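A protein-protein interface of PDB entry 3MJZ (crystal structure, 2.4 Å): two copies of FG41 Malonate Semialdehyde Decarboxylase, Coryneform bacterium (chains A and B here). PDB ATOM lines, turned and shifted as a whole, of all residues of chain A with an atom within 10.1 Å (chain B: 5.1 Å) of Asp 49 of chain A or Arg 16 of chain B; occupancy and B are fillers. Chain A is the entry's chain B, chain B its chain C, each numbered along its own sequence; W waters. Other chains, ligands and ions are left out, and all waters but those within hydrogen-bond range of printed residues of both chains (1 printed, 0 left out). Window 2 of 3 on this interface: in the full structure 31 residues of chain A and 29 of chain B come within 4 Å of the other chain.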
ATOM      1  N   ASP A   6     -22.374  18.461 -28.124  1.00  0.00           N
ATOM      2  CA  ASP A   6     -21.801  17.507 -27.212  1.00  0.00           C
ATOM      3  C   ASP A   6     -20.492  18.044 -26.685  1.00  0.00           C
ATOM      4  O   ASP A   6     -19.572  18.325 -27.444  1.00  0.00           O
ATOM      5  CB  ASP A   6     -21.626  16.147 -27.883  1.00  0.00           C
ATOM      6  CG  ASP A   6     -22.939  15.451 -28.094  1.00  0.00           C
ATOM      7  OD1 ASP A   6     -23.339  14.617 -27.242  1.00  0.00           O
ATOM      8  OD2 ASP A   6     -23.591  15.759 -29.113  1.00  0.00           O
ATOM      9  N   LEU A   7     -20.438  18.197 -25.365  1.00  0.00           N
ATOM     10  CA  LEU A   7     -19.292  18.800 -24.700  1.00  0.00           C
ATOM     11  C   LEU A   7     -18.969  18.020 -23.434  1.00  0.00           C
ATOM     12  O   LEU A   7     -19.599  16.998 -23.153  1.00  0.00           O
ATOM     13  CB  LEU A   7     -19.558  20.287 -24.405  1.00  0.00           C
ATOM     14  CG  LEU A   7     -20.939  20.729 -23.884  1.00  0.00           C
ATOM     15  CD1 LEU A   7     -21.147  20.314 -22.448  1.00  0.00           C
ATOM     16  CD2 LEU A   7     -21.104  22.240 -24.021  1.00  0.00           C
ATOM     17  N   THR A   8     -18.011  18.527 -22.664  1.00  0.00           N
ATOM     18  CA  THR A   8     -17.556  17.885 -21.444  1.00  0.00           C
ATOM     19  C   THR A   8     -18.158  18.478 -20.159  1.00  0.00           C
ATOM     20  O   THR A   8     -18.417  19.671 -20.084  1.00  0.00           O
ATOM     21  CB  THR A   8     -16.010  17.879 -21.393  1.00  0.00           C
ATOM     22  OG1 THR A   8     -15.502  19.231 -21.369  1.00  0.00           O
ATOM     23  CG2 THR A   8     -15.467  17.111 -22.615  1.00  0.00           C
ATOM     24  N   SER A   9     -18.357  17.602 -19.164  1.00  0.00           N
ATOM     25  CA  SER A   9     -18.945  17.905 -17.851  1.00  0.00           C
ATOM     26  C   SER A   9     -18.182  18.893 -16.983  1.00  0.00           C
ATOM     27  O   SER A   9     -18.714  19.362 -15.955  1.00  0.00           O
ATOM     28  CB  SER A   9     -19.044  16.646 -17.016  1.00  0.00           C
ATOM     29  OG  SER A   9     -19.589  15.591 -17.751  1.00  0.00           O
ATOM     30  N   ASP A  10     -16.937  19.181 -17.355  1.00  0.00           N
ATOM     31  CA  ASP A  10     -16.086  20.040 -16.543  1.00  0.00           C
ATOM     32  C   ASP A  10     -16.309  21.499 -16.873  1.00  0.00           C
ATOM     33  O   ASP A  10     -15.876  22.380 -16.140  1.00  0.00           O
ATOM     34  CB  ASP A  10     -14.622  19.632 -16.684  1.00  0.00           C
ATOM     35  CG  ASP A  10     -14.302  18.372 -15.899  1.00  0.00           C
ATOM     36  OD1 ASP A  10     -14.431  18.394 -14.646  1.00  0.00           O
ATOM     37  OD2 ASP A  10     -13.953  17.348 -16.538  1.00  0.00           O
ATOM     38  N   THR A  43     -25.539  17.928 -24.330  1.00  0.00           N
ATOM     39  CA  THR A  43     -25.230  16.703 -23.637  1.00  0.00           C
ATOM     40  C   THR A  43     -23.805  16.843 -23.127  1.00  0.00           C
ATOM     41  O   THR A  43     -22.885  17.144 -23.888  1.00  0.00           O
ATOM     42  CB  THR A  43     -25.378  15.490 -24.583  1.00  0.00           C
ATOM     43  OG1 THR A  43     -26.589  15.610 -25.371  1.00  0.00           O
ATOM     44  CG2 THR A  43     -25.396  14.200 -23.809  1.00  0.00           C
ATOM     45  N   ALA A  44     -23.626  16.655 -21.829  1.00  0.00           N
ATOM     46  CA  ALA A  44     -22.307  16.695 -21.222  1.00  0.00           C
ATOM     47  C   ALA A  44     -21.774  15.277 -21.007  1.00  0.00           C
ATOM     48  O   ALA A  44     -22.537  14.382 -20.619  1.00  0.00           O
ATOM     49  CB  ALA A  44     -22.345  17.475 -19.924  1.00  0.00           C
ATOM     50  N   HIS A  45     -20.482  15.088 -21.299  1.00  0.00           N
ATOM     51  CA  HIS A  45     -19.798  13.784 -21.226  1.00  0.00           C
ATOM     52  C   HIS A  45     -18.506  13.920 -20.441  1.00  0.00           C
ATOM     53  O   HIS A  45     -17.901  14.980 -20.439  1.00  0.00           O
ATOM     54  CB  HIS A  45     -19.401  13.264 -22.626  1.00  0.00           C
ATOM     55  CG  HIS A  45     -20.523  13.237 -23.609  1.00  0.00           C
ATOM     56  ND1 HIS A  45     -21.353  12.149 -23.768  1.00  0.00           N
ATOM     57  CD2 HIS A  45     -20.959  14.173 -24.487  1.00  0.00           C
ATOM     58  CE1 HIS A  45     -22.264  12.422 -24.687  1.00  0.00           C
ATOM     59  NE2 HIS A  45     -22.038  13.641 -25.147  1.00  0.00           N
ATOM     60  N   ASP A  46     -18.068  12.836 -19.796  1.00  0.00           N
ATOM     61  CA  ASP A  46     -16.689  12.712 -19.316  1.00  0.00           C
ATOM     62  C   ASP A  46     -15.745  12.814 -20.539  1.00  0.00           C
ATOM     63  O   ASP A  46     -15.974  12.131 -21.539  1.00  0.00           O
ATOM     64  CB  ASP A  46     -16.514  11.377 -18.577  1.00  0.00           C
ATOM     65  CG  ASP A  46     -15.143  11.243 -17.906  1.00  0.00           C
ATOM     66  OD1 ASP A  46     -15.013  11.618 -16.721  1.00  0.00           O
ATOM     67  OD2 ASP A  46     -14.185  10.769 -18.564  1.00  0.00           O
ATOM     68  N   PRO A  47     -14.689  13.668 -20.464  1.00  0.00           N
ATOM     69  CA  PRO A  47     -13.796  13.931 -21.617  1.00  0.00           C
ATOM     70  C   PRO A  47     -13.368  12.663 -22.373  1.00  0.00           C
ATOM     71  O   PRO A  47     -12.911  12.758 -23.507  1.00  0.00           O
ATOM     72  CB  PRO A  47     -12.578  14.583 -20.976  1.00  0.00           C
ATOM     73  CG  PRO A  47     -13.111  15.251 -19.767  1.00  0.00           C
ATOM     74  CD  PRO A  47     -14.260  14.421 -19.269  1.00  0.00           C
ATOM     75  N   SER A  48     -13.540  11.503 -21.732  1.00  0.00           N
ATOM     76  CA  SER A  48     -13.182  10.191 -22.249  1.00  0.00           C
ATOM     77  C   SER A  48     -14.172   9.631 -23.248  1.00  0.00           C
ATOM     78  O   SER A  48     -13.836   8.758 -24.042  1.00  0.00           O
ATOM     79  CB  SER A  48     -13.070   9.202 -21.068  1.00  0.00           C
ATOM     80  OG  SER A  48     -11.698   8.915 -20.829  1.00  0.00           O
ATOM     81  N   ASP A  49     -15.408  10.102 -23.164  1.00  0.00           N
ATOM     82  CA  ASP A  49     -16.458   9.627 -24.035  1.00  0.00           C
ATOM     83  C   ASP A  49     -16.645  10.495 -25.268  1.00  0.00           C
ATOM     84  O   ASP A  49     -17.560  10.252 -26.050  1.00  0.00           O
ATOM     85  CB  ASP A  49     -17.773   9.492 -23.273  1.00  0.00           C
ATOM     86  CG  ASP A  49     -17.682   8.513 -22.123  1.00  0.00           C
ATOM     87  OD1 ASP A  49     -16.937   7.502 -22.210  1.00  0.00           O
ATOM     88  OD2 ASP A  49     -18.350   8.785 -21.104  1.00  0.00           O
ATOM     89  N   ILE A  50     -15.777  11.496 -25.429  1.00  0.00           N
ATOM     90  CA  ILE A  50     -15.667  12.256 -26.667  1.00  0.00           C
ATOM     91  C   ILE A  50     -14.268  12.093 -27.221  1.00  0.00           C
ATOM     92  O   ILE A  50     -13.272  12.525 -26.595  1.00  0.00           O
ATOM     93  CB  ILE A  50     -15.933  13.766 -26.499  1.00  0.00           C
ATOM     94  CG1 ILE A  50     -17.319  14.020 -25.919  1.00  0.00           C
ATOM     95  CG2 ILE A  50     -15.788  14.467 -27.859  1.00  0.00           C
ATOM     96  CD1 ILE A  50     -17.508  15.442 -25.466  1.00  0.00           C
ATOM     97  N   ILE A  51     -14.211  11.461 -28.401  1.00  0.00           N
ATOM     98  CA  ILE A  51     -12.968  11.169 -29.062  1.00  0.00           C
ATOM     99  C   ILE A  51     -12.959  11.904 -30.383  1.00  0.00           C
ATOM    100  O   ILE A  51     -13.754  11.625 -31.289  1.00  0.00           O
ATOM    101  CB  ILE A  51     -12.765   9.665 -29.268  1.00  0.00           C
ATOM    102  CG1 ILE A  51     -12.976   8.921 -27.938  1.00  0.00           C
ATOM    103  CG2 ILE A  51     -11.375   9.402 -29.877  1.00  0.00           C
ATOM    104  CD1 ILE A  51     -13.179   7.432 -28.064  1.00  0.00           C
ATOM    105  N   ALA A  52     -12.051  12.866 -30.461  1.00  0.00           N
ATOM    106  CA  ALA A  52     -11.936  13.781 -31.584  1.00  0.00           C
ATOM    107  C   ALA A  52     -10.459  14.028 -31.795  1.00  0.00           C
ATOM    108  O   ALA A  52      -9.832  14.762 -31.015  1.00  0.00           O
ATOM    109  CB  ALA A  52     -12.653  15.101 -31.278  1.00  0.00           C
ATOM    110  N   PRO A  63      -8.621  18.125 -23.923  1.00  0.00           N
ATOM    111  CA  PRO A  63      -9.750  17.284 -23.563  1.00  0.00           C
ATOM    112  C   PRO A  63     -11.118  17.987 -23.680  1.00  0.00           C
ATOM    113  O   PRO A  63     -12.162  17.308 -23.720  1.00  0.00           O
ATOM    114  CB  PRO A  63      -9.449  16.959 -22.103  1.00  0.00           C
ATOM    115  CG  PRO A  63      -7.979  17.008 -22.021  1.00  0.00           C
ATOM    116  CD  PRO A  63      -7.649  18.203 -22.808  1.00  0.00           C
ATOM    117  N   VAL A  65     -13.270  19.278 -25.659  1.00  0.00           N
ATOM    118  CA  VAL A  65     -13.725  19.403 -27.041  1.00  0.00           C
ATOM    119  C   VAL A  65     -15.239  19.590 -27.123  1.00  0.00           C
ATOM    120  O   VAL A  65     -15.977  19.120 -26.252  1.00  0.00           O
ATOM    121  CB  VAL A  65     -13.107  18.287 -28.012  1.00  0.00           C
ATOM    122  CG1 VAL A  65     -12.660  17.083 -27.274  1.00  0.00           C
ATOM    123  CG2 VAL A  65     -14.050  17.912 -29.162  1.00  0.00           C
ATOM    124  N   ILE A  67     -18.407  19.281 -29.902  1.00  0.00           N
ATOM    125  CA  ILE A  67     -18.881  18.801 -31.185  1.00  0.00           C
ATOM    126  C   ILE A  67     -20.270  19.377 -31.427  1.00  0.00           C
ATOM    127  O   ILE A  67     -21.195  19.169 -30.637  1.00  0.00           O
ATOM    128  CB  ILE A  67     -18.908  17.278 -31.242  1.00  0.00           C
ATOM    129  CG1 ILE A  67     -17.481  16.764 -31.269  1.00  0.00           C
ATOM    130  CG2 ILE A  67     -19.668  16.787 -32.499  1.00  0.00           C
ATOM    131  CD1 ILE A  67     -17.276  15.558 -30.426  1.00  0.00           C
ATOM    132  N   LEU B   7     -24.864   3.254 -25.874  1.00  0.00           N
ATOM    133  CA  LEU B   7     -24.806   1.952 -25.249  1.00  0.00           C
ATOM    134  C   LEU B   7     -25.301   1.984 -23.778  1.00  0.00           C
ATOM    135  O   LEU B   7     -25.845   2.987 -23.315  1.00  0.00           O
ATOM    136  CB  LEU B   7     -23.388   1.375 -25.399  1.00  0.00           C
ATOM    137  CG  LEU B   7     -22.122   1.828 -24.666  1.00  0.00           C
ATOM    138  CD1 LEU B   7     -20.964   1.210 -25.386  1.00  0.00           C
ATOM    139  CD2 LEU B   7     -21.923   3.317 -24.635  1.00  0.00           C
ATOM    140  N   SER B   9     -24.888   1.548 -19.527  1.00  0.00           N
ATOM    141  CA  SER B   9     -23.893   2.031 -18.535  1.00  0.00           C
ATOM    142  C   SER B   9     -23.348   0.936 -17.603  1.00  0.00           C
ATOM    143  O   SER B   9     -22.462   1.180 -16.782  1.00  0.00           O
ATOM    144  CB  SER B   9     -24.470   3.183 -17.720  1.00  0.00           C
ATOM    145  OG  SER B   9     -25.682   2.802 -17.121  1.00  0.00           O
ATOM    146  N   ARG B  11     -21.875  -1.711 -18.820  1.00  0.00           N
ATOM    147  CA  ARG B  11     -20.565  -2.064 -19.358  1.00  0.00           C
ATOM    148  C   ARG B  11     -19.503  -1.186 -18.681  1.00  0.00           C
ATOM    149  O   ARG B  11     -19.755  -0.006 -18.434  1.00  0.00           O
ATOM    150  CB  ARG B  11     -20.503  -1.873 -20.873  1.00  0.00           C
ATOM    151  CG  ARG B  11     -21.548  -2.628 -21.660  1.00  0.00           C
ATOM    152  CD  ARG B  11     -21.184  -2.696 -23.127  1.00  0.00           C
ATOM    153  NE  ARG B  11     -22.163  -3.442 -23.922  1.00  0.00           N
ATOM    154  CZ  ARG B  11     -21.988  -4.697 -24.335  1.00  0.00           C
ATOM    155  NH1 ARG B  11     -20.887  -5.348 -24.002  1.00  0.00           N
ATOM    156  NH2 ARG B  11     -22.913  -5.313 -25.067  1.00  0.00           N
ATOM    157  N   SER B  12     -18.323  -1.758 -18.402  1.00  0.00           N
ATOM    158  CA  SER B  12     -17.238  -1.012 -17.778  1.00  0.00           C
ATOM    159  C   SER B  12     -16.729   0.111 -18.712  1.00  0.00           C
ATOM    160  O   SER B  12     -17.032   0.118 -19.927  1.00  0.00           O
ATOM    161  CB  SER B  12     -16.113  -1.962 -17.361  1.00  0.00           C
ATOM    162  OG  SER B  12     -15.418  -2.526 -18.469  1.00  0.00           O
ATOM    163  N   ARG B  13     -15.977   1.067 -18.153  1.00  0.00           N
ATOM    164  CA  ARG B  13     -15.419   2.150 -18.970  1.00  0.00           C
ATOM    165  C   ARG B  13     -14.447   1.570 -19.984  1.00  0.00           C
ATOM    166  O   ARG B  13     -14.460   1.960 -21.129  1.00  0.00           O
ATOM    167  CB  ARG B  13     -14.759   3.254 -18.123  1.00  0.00           C
ATOM    168  CG  ARG B  13     -15.681   3.926 -17.075  1.00  0.00           C
ATOM    169  CD  ARG B  13     -15.361   3.415 -15.639  1.00  0.00           C
ATOM    170  NE  ARG B  13     -16.286   2.383 -15.124  1.00  0.00           N
ATOM    171  CZ  ARG B  13     -15.968   1.124 -14.805  1.00  0.00           C
ATOM    172  NH1 ARG B  13     -14.732   0.665 -14.935  1.00  0.00           N
ATOM    173  NH2 ARG B  13     -16.913   0.317 -14.341  1.00  0.00           N
ATOM    174  N   GLU B  14     -13.633   0.622 -19.534  1.00  0.00           N
ATOM    175  CA  GLU B  14     -12.694  -0.109 -20.363  1.00  0.00           C
ATOM    176  C   GLU B  14     -13.324  -0.809 -21.592  1.00  0.00           C
ATOM    177  O   GLU B  14     -12.832  -0.661 -22.713  1.00  0.00           O
ATOM    178  CB  GLU B  14     -11.951  -1.128 -19.496  1.00  0.00           C
ATOM    179  CG  GLU B  14     -10.479  -1.274 -19.841  1.00  0.00           C
ATOM    180  CD  GLU B  14      -9.805  -2.457 -19.143  1.00  0.00           C
ATOM    181  OE1 GLU B  14      -9.231  -3.306 -19.867  1.00  0.00           O
ATOM    182  OE2 GLU B  14      -9.833  -2.536 -17.884  1.00  0.00           O
ATOM    183  N   GLN B  15     -14.400  -1.571 -21.380  1.00  0.00           N
ATOM    184  CA  GLN B  15     -15.122  -2.223 -22.478  1.00  0.00           C
ATOM    185  C   GLN B  15     -15.775  -1.190 -23.395  1.00  0.00           C
ATOM    186  O   GLN B  15     -15.785  -1.346 -24.633  1.00  0.00           O
ATOM    187  CB  GLN B  15     -16.160  -3.229 -21.942  1.00  0.00           C
ATOM    188  CG  GLN B  15     -16.915  -4.005 -23.019  1.00  0.00           C
ATOM    189  CD  GLN B  15     -17.783  -5.111 -22.454  1.00  0.00           C
ATOM    190  OE1 GLN B  15     -18.867  -4.861 -21.939  1.00  0.00           O
ATOM    191  NE2 GLN B  15     -17.307  -6.339 -22.545  1.00  0.00           N
ATOM    192  N   ARG B  16     -16.297  -0.137 -22.774  1.00  0.00           N
ATOM    193  CA  ARG B  16     -16.890   1.017 -23.470  1.00  0.00           C
ATOM    194  C   ARG B  16     -15.921   1.596 -24.516  1.00  0.00           C
ATOM    195  O   ARG B  16     -16.251   1.741 -25.701  1.00  0.00           O
ATOM    196  CB  ARG B  16     -17.289   2.062 -22.405  1.00  0.00           C
ATOM    197  CG  ARG B  16     -18.504   2.922 -22.675  1.00  0.00           C
ATOM    198  CD  ARG B  16     -18.611   4.080 -21.617  1.00  0.00           C
ATOM    199  NE  ARG B  16     -19.045   3.539 -20.316  1.00  0.00           N
ATOM    200  CZ  ARG B  16     -19.656   4.239 -19.355  1.00  0.00           C
ATOM    201  NH1 ARG B  16     -19.914   5.537 -19.509  1.00  0.00           N
ATOM    202  NH2 ARG B  16     -20.009   3.635 -18.232  1.00  0.00           N
ATOM    203  N   ARG B  17     -14.711   1.900 -24.064  1.00  0.00           N
ATOM    204  CA  ARG B  17     -13.603   2.331 -24.916  1.00  0.00           C
ATOM    205  C   ARG B  17     -13.186   1.285 -25.943  1.00  0.00           C
ATOM    206  O   ARG B  17     -12.907   1.642 -27.084  1.00  0.00           O
ATOM    207  CB  ARG B  17     -12.396   2.705 -24.061  1.00  0.00           C
ATOM    208  CG  ARG B  17     -11.197   3.218 -24.860  1.00  0.00           C
ATOM    209  CD  ARG B  17     -11.625   4.383 -25.758  1.00  0.00           C
ATOM    210  NE  ARG B  17     -10.505   5.200 -26.239  1.00  0.00           N
ATOM    211  CZ  ARG B  17     -10.118   6.357 -25.682  1.00  0.00           C
ATOM    212  NH1 ARG B  17     -10.741   6.853 -24.596  1.00  0.00           N
ATOM    213  NH2 ARG B  17      -9.100   7.029 -26.221  1.00  0.00           N
ATOM    214  N   ALA B  18     -13.131   0.010 -25.549  1.00  0.00           N
ATOM    215  CA  ALA B  18     -12.791  -1.068 -26.473  1.00  0.00           C
ATOM    216  C   ALA B  18     -13.816  -1.199 -27.615  1.00  0.00           C
ATOM    217  O   ALA B  18     -13.437  -1.465 -28.752  1.00  0.00           O
ATOM    218  CB  ALA B  18     -12.609  -2.403 -25.728  1.00  0.00           C
ATOM    219  N   ILE B  19     -15.102  -0.998 -27.308  1.00  0.00           N
ATOM    220  CA  ILE B  19     -16.175  -0.863 -28.329  1.00  0.00           C
ATOM    221  C   ILE B  19     -15.866   0.275 -29.322  1.00  0.00           C
ATOM    222  O   ILE B  19     -16.035   0.110 -30.536  1.00  0.00           O
ATOM    223  CB  ILE B  19     -17.577  -0.701 -27.670  1.00  0.00           C
ATOM    224  CG1 ILE B  19     -18.022  -2.031 -27.040  1.00  0.00           C
ATOM    225  CG2 ILE B  19     -18.632  -0.252 -28.647  1.00  0.00           C
ATOM    226  CD1 ILE B  19     -18.955  -1.889 -25.816  1.00  0.00           C
ATOM    227  N   ALA B  20     -15.385   1.410 -28.802  1.00  0.00           N
ATOM    228  CA  ALA B  20     -15.099   2.586 -29.615  1.00  0.00           C
ATOM    229  C   ALA B  20     -13.912   2.335 -30.505  1.00  0.00           C
ATOM    230  O   ALA B  20     -13.907   2.773 -31.668  1.00  0.00           O
ATOM    231  CB  ALA B  20     -14.832   3.766 -28.745  1.00  0.00           C
ATOM    232  N   GLN B  40     -15.867  10.373 -32.459  1.00  0.00           N
ATOM    233  CA  GLN B  40     -16.793   9.504 -31.754  1.00  0.00           C
ATOM    234  C   GLN B  40     -17.352  10.153 -30.494  1.00  0.00           C
ATOM    235  O   GLN B  40     -16.624  10.730 -29.698  1.00  0.00           O
ATOM    236  CB  GLN B  40     -16.102   8.189 -31.389  1.00  0.00           C
ATOM    237  CG  GLN B  40     -15.575   7.391 -32.578  1.00  0.00           C
ATOM    238  CD  GLN B  40     -14.852   6.129 -32.139  1.00  0.00           C
ATOM    239  OE1 GLN B  40     -14.179   6.121 -31.101  1.00  0.00           O
ATOM    240  NE2 GLN B  40     -15.000   5.042 -32.915  1.00  0.00           N
ATOM    241  N   ILE B  41     -18.667  10.043 -30.341  1.00  0.00           N
ATOM    242  CA  ILE B  41     -19.365  10.391 -29.113  1.00  0.00           C
ATOM    243  C   ILE B  41     -19.997   9.121 -28.501  1.00  0.00           C
ATOM    244  O   ILE B  41     -20.900   8.528 -29.091  1.00  0.00           O
ATOM    245  CB  ILE B  41     -20.410  11.512 -29.356  1.00  0.00           C
ATOM    246  CG1 ILE B  41     -19.721  12.725 -29.965  1.00  0.00           C
ATOM    247  CG2 ILE B  41     -21.112  11.914 -28.039  1.00  0.00           C
ATOM    248  CD1 ILE B  41     -20.530  13.399 -31.007  1.00  0.00           C
ATOM    249  N   LEU B  42     -19.499   8.729 -27.320  1.00  0.00           N
ATOM    250  CA  LEU B  42     -19.986   7.587 -26.522  1.00  0.00           C
ATOM    251  C   LEU B  42     -21.016   8.057 -25.505  1.00  0.00           C
ATOM    252  O   LEU B  42     -20.711   8.931 -24.672  1.00  0.00           O
ATOM    253  CB  LEU B  42     -18.801   6.949 -25.776  1.00  0.00           C
ATOM    254  CG  LEU B  42     -17.779   6.053 -26.519  1.00  0.00           C
ATOM    255  CD1 LEU B  42     -17.402   6.567 -27.908  1.00  0.00           C
ATOM    256  CD2 LEU B  42     -16.500   5.759 -25.694  1.00  0.00           C
ATOM    257  N   ALA B  44     -23.548   6.461 -22.596  1.00  0.00           N
ATOM    258  CA  ALA B  44     -23.989   5.316 -21.810  1.00  0.00           C
ATOM    259  C   ALA B  44     -25.289   5.622 -21.088  1.00  0.00           C
ATOM    260  O   ALA B  44     -25.432   6.659 -20.430  1.00  0.00           O
ATOM    261  CB  ALA B  44     -22.915   4.891 -20.839  1.00  0.00           C
HETATM  262  O   HOH W   1     -20.726  10.025 -21.884  1.00  0.00           O
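Ser 9 of chain A touches none of the printed residues of chain B. Of the printed residues of chain B, His 45 of chain A touches Ile 41 and Leu 42. Of the printed residues of chain B, Ile 51 of chain A touches Arg 17 and Gln 40. Printed residues of chain B within 4 Å of Ile 67 of chain A: Ile 41. Leu 7 of chain B touches none of the printed residues of chain A. No residue of chain A comes within 4 Å of Ser 9 of chain B. Ser 12 of chain B touches none of the printed residues of chain A. Printed residues of chain A within 4 Å of Arg 16 of chain B: Asp 49 (3.9 Å). Of the printed residues of chain A, Arg 17 of chain B touches Ser 48 and Ile 51. No residue of chain A comes within 4 Å of Ala 18 of chain B. No residue of chain A comes within 4 Å of Ile 19 of chain B. Of chain A, only His 45 and Asp 49 come within 4 Å of Leu 42 of chain B. No residue of chain A comes within 4 Å of Ala 44 of chain B. The nearest printed residue of chain B that does not touch Asp 49 of chain A is Arg 17 of chain B (5.9 Å).
Water W1 lies within hydrogen-bond range of the side-chain carboxylate (OD2) of Asp 49 of chain A (2.8 Å), a ring nitrogen (ND1) of His 45 of chain A (2.9 Å) and the backbone carbonyl oxygen (O) of Leu 42 of chain B (3.0 Å).
N of Ser 9 of chain A sits at hydrogen-bond distance from O of His 45 of chain A, at 3.0 Å. The side-chain carboxylate (OD1) of Asp 6 of chain A sits at hydrogen-bond distance from a ring nitrogen (NE2) of His 45 of chain A (2.7 Å). The backbone carbonyl oxygen (O) of Leu 7 of chain A sits at hydrogen-bond distance from the backbone NH (N) of His 45 of chain A. N of Asp 6 of chain A lies within hydrogen-bond range of O of Ile 67 of chain A. The backbone NH (N) of Ser 48 of chain A sits close to the side-chain carboxylate (OD2) of Asp 46 of chain A, at 3.3 Å. The side-chain amide nitrogen (NE2) of Gln 40 of chain B lies within hydrogen-bond range of the backbone carbonyl oxygen (O) of Ala 20 of chain B.
Hydrophobic or aromatic side chains of chain B within 4 Å of the printed part of chain A: Ile 41 and Leu 42. Printed residues of chain A that touch a printed residue of chain B: Asp 6, His 45, Ser 48, Asp 49, Ile 50, Ile 51 and Ile 67. Among the printed residues, 12 pairs touch across the chains.
Positions printed for both chains: 7, 9 and 44. Of the 12 pairs that touch across the chains among the printed residues, none has its exchanged pair printed and touching as well.
Among the printed residues, pairs that only touch across the chains: His 45 of chain A with Ile 41 of chain B (3.5 Å), Ile 50 of chain A with Gln 40 of chain B (3.5 Å), Asp 49 of chain A with Ile 41 of chain B (3.6 Å), Asp 6 of chain A with Ile 41 of chain B (3.6 Å), Ser 48 of chain A with Arg 17 of chain B (3.7 Å), Ile 67 of chain A with Ile 41 of chain B (3.8 Å), Asp 49 of chain A with Gln 40 of chain B (3.8 Å) and Ile 51 of chain A with Arg 17 of chain B (3.9 Å).
The backbone carbonyl oxygen of Asp 49 of chain A sits at hydrogen-bond distance from the backbone NH of Leu 42 of chain B (2.8 Å). The guanidinium group of Arg 16 of chain B is in salt-bridge range of the side-chain carboxylate of Asp 49 of chain A, 3.9 Å away. The backbone carbonyl oxygen (O) of Ile 51 of chain A sits at hydrogen-bond distance from the backbone NH (N) of Gln 40 of chain B (2.7 Å). ND1 of His 45 of chain A lies within hydrogen-bond range of O of Leu 42 of chain B.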
